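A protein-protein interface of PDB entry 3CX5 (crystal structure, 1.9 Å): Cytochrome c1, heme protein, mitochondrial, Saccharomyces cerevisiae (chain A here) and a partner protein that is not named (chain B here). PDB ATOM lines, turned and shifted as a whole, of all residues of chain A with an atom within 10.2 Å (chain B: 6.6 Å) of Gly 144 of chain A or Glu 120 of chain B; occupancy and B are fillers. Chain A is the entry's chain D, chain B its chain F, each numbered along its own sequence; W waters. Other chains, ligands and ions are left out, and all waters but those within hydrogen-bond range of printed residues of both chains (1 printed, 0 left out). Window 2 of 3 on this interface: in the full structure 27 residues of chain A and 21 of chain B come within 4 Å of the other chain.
Of the 15 printed residues of chain B, 5 touch a printed residue of chain A. Hydrophobic or aromatic side chains of chain B that line the printed part of chain A: Tyr 97 and Val 104. Of the 11 printed residues of chain A, 3 touch a printed residue of chain B. Among the printed residues, no Asp or Glu carboxylate lies within 4 Å of a Lys or Arg side-chain nitrogen of the other chain.
Among the printed residues, pairs that only touch across the chains: Pro 142 of chain A with Tyr 97 of chain B (3.2 Å), Ala 143 of chain A with Asp 121 of chain B (3.2 Å), Gly 144 of chain A with Val 104 of chain B (3.8 Å), Gly 144 of chain A with Glu 120 of chain B (3.8 Å), Gly 144 of chain A with Asp 121 of chain B (3.9 Å) and Pro 142 of chain A with Cys 122 of chain B (3.99 Å).
The backbone carbonyl oxygen (O) of Ala 143 of chain A is in hydrogen-bond range of the backbone NH (N) of Cys 122 of chain B (2.8 Å). The backbone NH of Ala 143 of chain A is in hydrogen-bond range of the side-chain hydroxyl of Tyr 97 of chain B.
Water W1 lies within hydrogen-bond range of N of Gly 144 of chain A and OE1 of Gln 108 of chain B.
Of the printed residues of chain B, Pro 142 of chain A touches Tyr 97 and Cys 122. Of the printed residues of chain B, Ala 143 of chain A touches Tyr 97 (3.0 Å), Asp 121 (3.2 Å) and Cys 122 (2.8 Å). Of chain B, only Val 104 (3.8 Å), Glu 120 (3.8 Å) and Asp 121 (3.9 Å) come within 4 Å of Gly 144 of chain A. Tyr 153 of chain A touches none of the printed residues of chain B. Of the printed residues of chain A, Tyr 97 of chain B touches Pro 142 (3.2 Å) and Ala 143 (3.0 Å). Of chain A, only Gly 144 comes within 4 Å of Glu 120 of chain B. Of the printed residues of chain A, Asp 121 of chain B touches Ala 143 and Gly 144. Of the printed residues of chain A, Cys 122 of chain B touches Pro 142 and Ala 143.
The side-chain carboxylate (OE2) of Glu 120 of chain B lies within salt-bridge range of the guanidinium group (NH1) of Arg 103 of chain B (2.9 Å). NE2 of Gln 107 of chain B is in hydrogen-bond range of OE1 of Glu 120 of chain B, at 3.0 Å. The side-chain sulfur (SG) of Cys 100 of chain B forms a disulfide with the side-chain sulfur (SG) of Cys 122 of chain B (2.0 Å).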
ATOM      1  N   ALA A   4      15.142  -7.061  12.352  1.00  0.00           N
ATOM      2  CA  ALA A   4      15.402  -5.718  11.852  1.00  0.00           C
ATOM      3  C   ALA A   4      14.786  -5.500  10.462  1.00  0.00           C
ATOM      4  O   ALA A   4      14.171  -4.463  10.200  1.00  0.00           O
ATOM      5  CB  ALA A   4      16.902  -5.460  11.814  1.00  0.00           C
ATOM      6  N   GLU A 140      18.802   7.332  20.376  1.00  0.00           N
ATOM      7  CA  GLU A 140      19.946   6.787  19.651  1.00  0.00           C
ATOM      8  C   GLU A 140      19.647   5.392  19.107  1.00  0.00           C
ATOM      9  O   GLU A 140      18.840   4.651  19.673  1.00  0.00           O
ATOM     10  CB  GLU A 140      21.166   6.687  20.578  1.00  0.00           C
ATOM     11  CG  GLU A 140      21.744   8.016  21.056  1.00  0.00           C
ATOM     12  CD  GLU A 140      22.747   7.834  22.185  1.00  0.00           C
ATOM     13  OE1 GLU A 140      23.818   7.227  21.947  1.00  0.00           O
ATOM     14  OE2 GLU A 140      22.458   8.288  23.315  1.00  0.00           O
ATOM     15  N   PRO A 141      20.277   5.028  17.981  1.00  0.00           N
ATOM     16  CA  PRO A 141      20.069   3.705  17.387  1.00  0.00           C
ATOM     17  C   PRO A 141      20.781   2.668  18.254  1.00  0.00           C
ATOM     18  O   PRO A 141      21.710   3.004  18.989  1.00  0.00           O
ATOM     19  CB  PRO A 141      20.741   3.839  16.017  1.00  0.00           C
ATOM     20  CG  PRO A 141      21.833   4.832  16.268  1.00  0.00           C
ATOM     21  CD  PRO A 141      21.132   5.863  17.118  1.00  0.00           C
ATOM     22  N   PRO A 142      20.334   1.402  18.211  1.00  0.00           N
ATOM     23  CA  PRO A 142      20.980   0.365  19.020  1.00  0.00           C
ATOM     24  C   PRO A 142      22.443   0.181  18.631  1.00  0.00           C
ATOM     25  O   PRO A 142      22.828   0.458  17.493  1.00  0.00           O
ATOM     26  CB  PRO A 142      20.136  -0.881  18.725  1.00  0.00           C
ATOM     27  CG  PRO A 142      19.549  -0.603  17.378  1.00  0.00           C
ATOM     28  CD  PRO A 142      19.195   0.851  17.458  1.00  0.00           C
ATOM     29  N   ALA A 143      23.253  -0.255  19.595  1.00  0.00           N
ATOM     30  CA  ALA A 143      24.683  -0.464  19.384  1.00  0.00           C
ATOM     31  C   ALA A 143      24.994  -1.344  18.182  1.00  0.00           C
ATOM     32  O   ALA A 143      24.392  -2.404  18.006  1.00  0.00           O
ATOM     33  CB  ALA A 143      25.312  -1.055  20.635  1.00  0.00           C
ATOM     34  N   GLY A 144      25.933  -0.891  17.356  1.00  0.00           N
ATOM     35  CA  GLY A 144      26.321  -1.650  16.180  1.00  0.00           C
ATOM     36  C   GLY A 144      25.553  -1.324  14.910  1.00  0.00           C
ATOM     37  O   GLY A 144      25.898  -1.810  13.832  1.00  0.00           O
ATOM     38  N   VAL A 145      24.499  -0.523  15.033  1.00  0.00           N
ATOM     39  CA  VAL A 145      23.707  -0.140  13.875  1.00  0.00           C
ATOM     40  C   VAL A 145      24.360   1.020  13.130  1.00  0.00           C
ATOM     41  O   VAL A 145      24.474   2.132  13.651  1.00  0.00           O
ATOM     42  CB  VAL A 145      22.248   0.215  14.273  1.00  0.00           C
ATOM     43  CG1 VAL A 145      21.526   0.921  13.126  1.00  0.00           C
ATOM     44  CG2 VAL A 145      21.500  -1.054  14.641  1.00  0.00           C
ATOM     45  N   ALA A 146      24.829   0.728  11.922  1.00  0.00           N
ATOM     46  CA  ALA A 146      25.463   1.729  11.074  1.00  0.00           C
ATOM     47  C   ALA A 146      24.350   2.429  10.306  1.00  0.00           C
ATOM     48  O   ALA A 146      23.736   1.847   9.411  1.00  0.00           O
ATOM     49  CB  ALA A 146      26.446   1.066  10.112  1.00  0.00           C
ATOM     50  N   LEU A 147      24.083   3.676  10.677  1.00  0.00           N
ATOM     51  CA  LEU A 147      23.028   4.456  10.047  1.00  0.00           C
ATOM     52  C   LEU A 147      23.583   5.438   9.014  1.00  0.00           C
ATOM     53  O   LEU A 147      24.426   6.279   9.333  1.00  0.00           O
ATOM     54  CB  LEU A 147      22.258   5.214  11.126  1.00  0.00           C
ATOM     55  CG  LEU A 147      20.755   5.408  10.959  1.00  0.00           C
ATOM     56  CD1 LEU A 147      20.056   4.059  10.863  1.00  0.00           C
ATOM     57  CD2 LEU A 147      20.234   6.191  12.152  1.00  0.00           C
ATOM     58  N   PRO A 148      23.120   5.334   7.755  1.00  0.00           N
ATOM     59  CA  PRO A 148      23.563   6.214   6.665  1.00  0.00           C
ATOM     60  C   PRO A 148      23.261   7.676   6.990  1.00  0.00           C
ATOM     61  O   PRO A 148      22.232   7.981   7.593  1.00  0.00           O
ATOM     62  CB  PRO A 148      22.717   5.735   5.483  1.00  0.00           C
ATOM     63  CG  PRO A 148      22.496   4.284   5.787  1.00  0.00           C
ATOM     64  CD  PRO A 148      22.173   4.322   7.256  1.00  0.00           C
ATOM     65  N   TYR A 153      16.888   6.249  12.851  1.00  0.00           N
ATOM     66  CA  TYR A 153      16.527   4.925  13.316  1.00  0.00           C
ATOM     67  C   TYR A 153      15.140   4.856  13.942  1.00  0.00           C
ATOM     68  O   TYR A 153      14.791   5.662  14.803  1.00  0.00           O
ATOM     69  CB  TYR A 153      17.549   4.378  14.316  1.00  0.00           C
ATOM     70  CG  TYR A 153      17.235   2.958  14.716  1.00  0.00           C
ATOM     71  CD1 TYR A 153      17.666   1.888  13.936  1.00  0.00           C
ATOM     72  CD2 TYR A 153      16.453   2.683  15.840  1.00  0.00           C
ATOM     73  CE1 TYR A 153      17.325   0.584  14.260  1.00  0.00           C
ATOM     74  CE2 TYR A 153      16.104   1.378  16.171  1.00  0.00           C
ATOM     75  CZ  TYR A 153      16.547   0.338  15.374  1.00  0.00           C
ATOM     76  OH  TYR A 153      16.222  -0.952  15.697  1.00  0.00           O
ATOM     77  N   TYR B  97      20.643  -5.804  27.190  1.00  0.00           N
ATOM     78  CA  TYR B  97      20.952  -4.909  26.081  1.00  0.00           C
ATOM     79  C   TYR B  97      22.248  -4.159  26.389  1.00  0.00           C
ATOM     80  O   TYR B  97      23.112  -4.013  25.521  1.00  0.00           O
ATOM     81  CB  TYR B  97      19.825  -3.897  25.842  1.00  0.00           C
ATOM     82  CG  TYR B  97      20.226  -2.816  24.858  1.00  0.00           C
ATOM     83  CD1 TYR B  97      20.255  -3.072  23.484  1.00  0.00           C
ATOM     84  CD2 TYR B  97      20.667  -1.567  25.307  1.00  0.00           C
ATOM     85  CE1 TYR B  97      20.725  -2.118  22.584  1.00  0.00           C
ATOM     86  CE2 TYR B  97      21.140  -0.604  24.414  1.00  0.00           C
ATOM     87  CZ  TYR B  97      21.170  -0.888  23.055  1.00  0.00           C
ATOM     88  OH  TYR B  97      21.665   0.048  22.176  1.00  0.00           O
ATOM     89  N   CYS B 100      25.288  -6.190  25.747  1.00  0.00           N
ATOM     90  CA  CYS B 100      25.563  -6.272  24.311  1.00  0.00           C
ATOM     91  C   CYS B 100      26.212  -4.979  23.799  1.00  0.00           C
ATOM     92  O   CYS B 100      27.175  -5.020  23.031  1.00  0.00           O
ATOM     93  CB  CYS B 100      24.266  -6.556  23.534  1.00  0.00           C
ATOM     94  SG  CYS B 100      24.464  -6.633  21.719  1.00  0.00           S
ATOM     95  N   ARG B 103      29.861  -4.836  24.896  1.00  0.00           N
ATOM     96  CA  ARG B 103      30.602  -5.828  24.125  1.00  0.00           C
ATOM     97  C   ARG B 103      30.858  -5.346  22.698  1.00  0.00           C
ATOM     98  O   ARG B 103      31.917  -5.608  22.124  1.00  0.00           O
ATOM     99  CB  ARG B 103      29.833  -7.153  24.108  1.00  0.00           C
ATOM    100  CG  ARG B 103      30.486  -8.265  23.298  1.00  0.00           C
ATOM    101  CD  ARG B 103      29.726  -9.582  23.440  1.00  0.00           C
ATOM    102  NE  ARG B 103      28.378  -9.522  22.875  1.00  0.00           N
ATOM    103  CZ  ARG B 103      27.255  -9.678  23.576  1.00  0.00           C
ATOM    104  NH1 ARG B 103      26.079  -9.609  22.967  1.00  0.00           N
ATOM    105  NH2 ARG B 103      27.302  -9.891  24.885  1.00  0.00           N
ATOM    106  N   VAL B 104      29.895  -4.616  22.141  1.00  0.00           N
ATOM    107  CA  VAL B 104      30.009  -4.094  20.784  1.00  0.00           C
ATOM    108  C   VAL B 104      30.917  -2.868  20.694  1.00  0.00           C
ATOM    109  O   VAL B 104      31.651  -2.711  19.715  1.00  0.00           O
ATOM    110  CB  VAL B 104      28.610  -3.798  20.181  1.00  0.00           C
ATOM    111  CG1 VAL B 104      28.728  -3.003  18.885  1.00  0.00           C
ATOM    112  CG2 VAL B 104      27.886  -5.110  19.911  1.00  0.00           C
ATOM    113  N   GLN B 107      34.419  -4.000  20.435  1.00  0.00           N
ATOM    114  CA  GLN B 107      34.737  -4.560  19.122  1.00  0.00           C
ATOM    115  C   GLN B 107      35.076  -3.462  18.118  1.00  0.00           C
ATOM    116  O   GLN B 107      35.948  -3.638  17.265  1.00  0.00           O
ATOM    117  CB  GLN B 107      33.561  -5.374  18.582  1.00  0.00           C
ATOM    118  CG  GLN B 107      33.266  -6.658  19.333  1.00  0.00           C
ATOM    119  CD  GLN B 107      32.096  -7.418  18.730  1.00  0.00           C
ATOM    120  OE1 GLN B 107      31.912  -7.434  17.511  1.00  0.00           O
ATOM    121  NE2 GLN B 107      31.296  -8.050  19.583  1.00  0.00           N
ATOM    122  N   GLN B 108      34.377  -2.334  18.229  1.00  0.00           N
ATOM    123  CA  GLN B 108      34.575  -1.193  17.337  1.00  0.00           C
ATOM    124  C   GLN B 108      35.940  -0.526  17.501  1.00  0.00           C
ATOM    125  O   GLN B 108      36.466   0.062  16.554  1.00  0.00           O
ATOM    126  CB  GLN B 108      33.463  -0.159  17.546  1.00  0.00           C
ATOM    127  CG  GLN B 108      32.063  -0.689  17.261  1.00  0.00           C
ATOM    128  CD  GLN B 108      30.973   0.325  17.551  1.00  0.00           C
ATOM    129  OE1 GLN B 108      29.909   0.299  16.934  1.00  0.00           O
ATOM    130  NE2 GLN B 108      31.228   1.219  18.500  1.00  0.00           N
ATOM    131  N   TYR B 113      38.448  -3.505  12.431  1.00  0.00           N
ATOM    132  CA  TYR B 113      37.016  -3.668  12.662  1.00  0.00           C
ATOM    133  C   TYR B 113      36.204  -3.426  11.391  1.00  0.00           C
ATOM    134  O   TYR B 113      35.207  -4.106  11.149  1.00  0.00           O
ATOM    135  CB  TYR B 113      36.544  -2.717  13.770  1.00  0.00           C
ATOM    136  CG  TYR B 113      35.040  -2.672  13.941  1.00  0.00           C
ATOM    137  CD1 TYR B 113      34.304  -1.563  13.522  1.00  0.00           C
ATOM    138  CD2 TYR B 113      34.350  -3.747  14.498  1.00  0.00           C
ATOM    139  CE1 TYR B 113      32.919  -1.527  13.652  1.00  0.00           C
ATOM    140  CE2 TYR B 113      32.963  -3.721  14.633  1.00  0.00           C
ATOM    141  CZ  TYR B 113      32.255  -2.610  14.208  1.00  0.00           C
ATOM    142  OH  TYR B 113      30.886  -2.584  14.334  1.00  0.00           O
ATOM    143  N   LEU B 116      35.893  -6.430   9.338  1.00  0.00           N
ATOM    144  CA  LEU B 116      35.390  -7.578  10.089  1.00  0.00           C
ATOM    145  C   LEU B 116      34.202  -8.231   9.379  1.00  0.00           C
ATOM    146  O   LEU B 116      33.979  -9.436   9.516  1.00  0.00           O
ATOM    147  CB  LEU B 116      35.008  -7.154  11.512  1.00  0.00           C
ATOM    148  CG  LEU B 116      35.121  -8.178  12.649  1.00  0.00           C
ATOM    149  CD1 LEU B 116      35.078  -7.461  13.989  1.00  0.00           C
ATOM    150  CD2 LEU B 116      34.023  -9.228  12.568  1.00  0.00           C
ATOM    151  N   GLU B 117      33.462  -7.430   8.610  1.00  0.00           N
ATOM    152  CA  GLU B 117      32.290  -7.891   7.853  1.00  0.00           C
ATOM    153  C   GLU B 117      31.096  -8.239   8.746  1.00  0.00           C
ATOM    154  O   GLU B 117      30.082  -7.537   8.728  1.00  0.00           O
ATOM    155  CB  GLU B 117      32.657  -9.081   6.958  1.00  0.00           C
ATOM    156  CG  GLU B 117      31.529  -9.575   6.064  1.00  0.00           C
ATOM    157  CD  GLU B 117      31.960 -10.720   5.167  1.00  0.00           C
ATOM    158  OE1 GLU B 117      31.377 -11.820   5.282  1.00  0.00           O
ATOM    159  OE2 GLU B 117      32.881 -10.521   4.346  1.00  0.00           O
ATOM    160  N   HIS B 118      31.210  -9.328   9.505  1.00  0.00           N
ATOM    161  CA  HIS B 118      30.143  -9.757  10.411  1.00  0.00           C
ATOM    162  C   HIS B 118      30.209  -8.983  11.723  1.00  0.00           C
ATOM    163  O   HIS B 118      30.621  -9.513  12.757  1.00  0.00           O
ATOM    164  CB  HIS B 118      30.230 -11.260  10.677  1.00  0.00           C
ATOM    165  CG  HIS B 118      29.935 -12.101   9.475  1.00  0.00           C
ATOM    166  ND1 HIS B 118      30.872 -12.933   8.900  1.00  0.00           N
ATOM    167  CD2 HIS B 118      28.809 -12.231   8.735  1.00  0.00           C
ATOM    168  CE1 HIS B 118      30.335 -13.538   7.855  1.00  0.00           C
ATOM    169  NE2 HIS B 118      29.085 -13.129   7.733  1.00  0.00           N
ATOM    170  N   LYS B 119      29.809  -7.717  11.660  1.00  0.00           N
ATOM    171  CA  LYS B 119      29.816  -6.838  12.822  1.00  0.00           C
ATOM    172  C   LYS B 119      28.535  -7.041  13.624  1.00  0.00           C
ATOM    173  O   LYS B 119      27.433  -6.859  13.107  1.00  0.00           O
ATOM    174  CB  LYS B 119      29.939  -5.379  12.373  1.00  0.00           C
ATOM    175  CG  LYS B 119      30.975  -5.164  11.278  1.00  0.00           C
ATOM    176  CD  LYS B 119      31.111  -3.701  10.888  1.00  0.00           C
ATOM    177  CE  LYS B 119      31.835  -3.553   9.554  1.00  0.00           C
ATOM    178  NZ  LYS B 119      33.099  -4.339   9.497  1.00  0.00           N
ATOM    179  N   GLU B 120      28.691  -7.440  14.881  1.00  0.00           N
ATOM    180  CA  GLU B 120      27.553  -7.675  15.757  1.00  0.00           C
ATOM    181  C   GLU B 120      26.830  -6.383  16.126  1.00  0.00           C
ATOM    182  O   GLU B 120      27.448  -5.328  16.264  1.00  0.00           O
ATOM    183  CB  GLU B 120      28.005  -8.383  17.036  1.00  0.00           C
ATOM    184  CG  GLU B 120      26.881  -8.616  18.041  1.00  0.00           C
ATOM    185  CD  GLU B 120      27.345  -9.252  19.339  1.00  0.00           C
ATOM    186  OE1 GLU B 120      28.567  -9.278  19.608  1.00  0.00           O
ATOM    187  OE2 GLU B 120      26.475  -9.724  20.102  1.00  0.00           O
ATOM    188  N   ASP B 121      25.510  -6.473  16.251  1.00  0.00           N
ATOM    189  CA  ASP B 121      24.686  -5.332  16.628  1.00  0.00           C
ATOM    190  C   ASP B 121      23.753  -5.777  17.752  1.00  0.00           C
ATOM    191  O   ASP B 121      23.619  -6.971  18.017  1.00  0.00           O
ATOM    192  CB  ASP B 121      23.892  -4.806  15.431  1.00  0.00           C
ATOM    193  CG  ASP B 121      23.016  -5.863  14.805  1.00  0.00           C
ATOM    194  OD1 ASP B 121      23.530  -6.636  13.966  1.00  0.00           O
ATOM    195  OD2 ASP B 121      21.822  -5.931  15.165  1.00  0.00           O
ATOM    196  N   CYS B 122      23.091  -4.822  18.392  1.00  0.00           N
ATOM    197  CA  CYS B 122      22.207  -5.138  19.504  1.00  0.00           C
ATOM    198  C   CYS B 122      20.716  -4.894  19.241  1.00  0.00           C
ATOM    199  O   CYS B 122      19.950  -4.598  20.165  1.00  0.00           O
ATOM    200  CB  CYS B 122      22.682  -4.380  20.750  1.00  0.00           C
ATOM    201  SG  CYS B 122      24.444  -4.684  21.149  1.00  0.00           S
ATOM    202  N   GLU B 125      18.431  -7.551  21.068  1.00  0.00           N
ATOM    203  CA  GLU B 125      18.300  -7.276  22.499  1.00  0.00           C
ATOM    204  C   GLU B 125      17.390  -6.076  22.696  1.00  0.00           C
ATOM    205  O   GLU B 125      16.599  -6.032  23.637  1.00  0.00           O
ATOM    206  CB  GLU B 125      19.666  -7.003  23.144  1.00  0.00           C
ATOM    207  CG  GLU B 125      20.584  -8.223  23.255  1.00  0.00           C
ATOM    208  CD  GLU B 125      21.239  -8.622  21.938  1.00  0.00           C
ATOM    209  OE1 GLU B 125      21.153  -7.864  20.948  1.00  0.00           O
ATOM    210  OE2 GLU B 125      21.859  -9.700  21.898  1.00  0.00           O
HETATM  211  O   HOH W   1      27.301   1.829  18.048  1.00  0.00           O
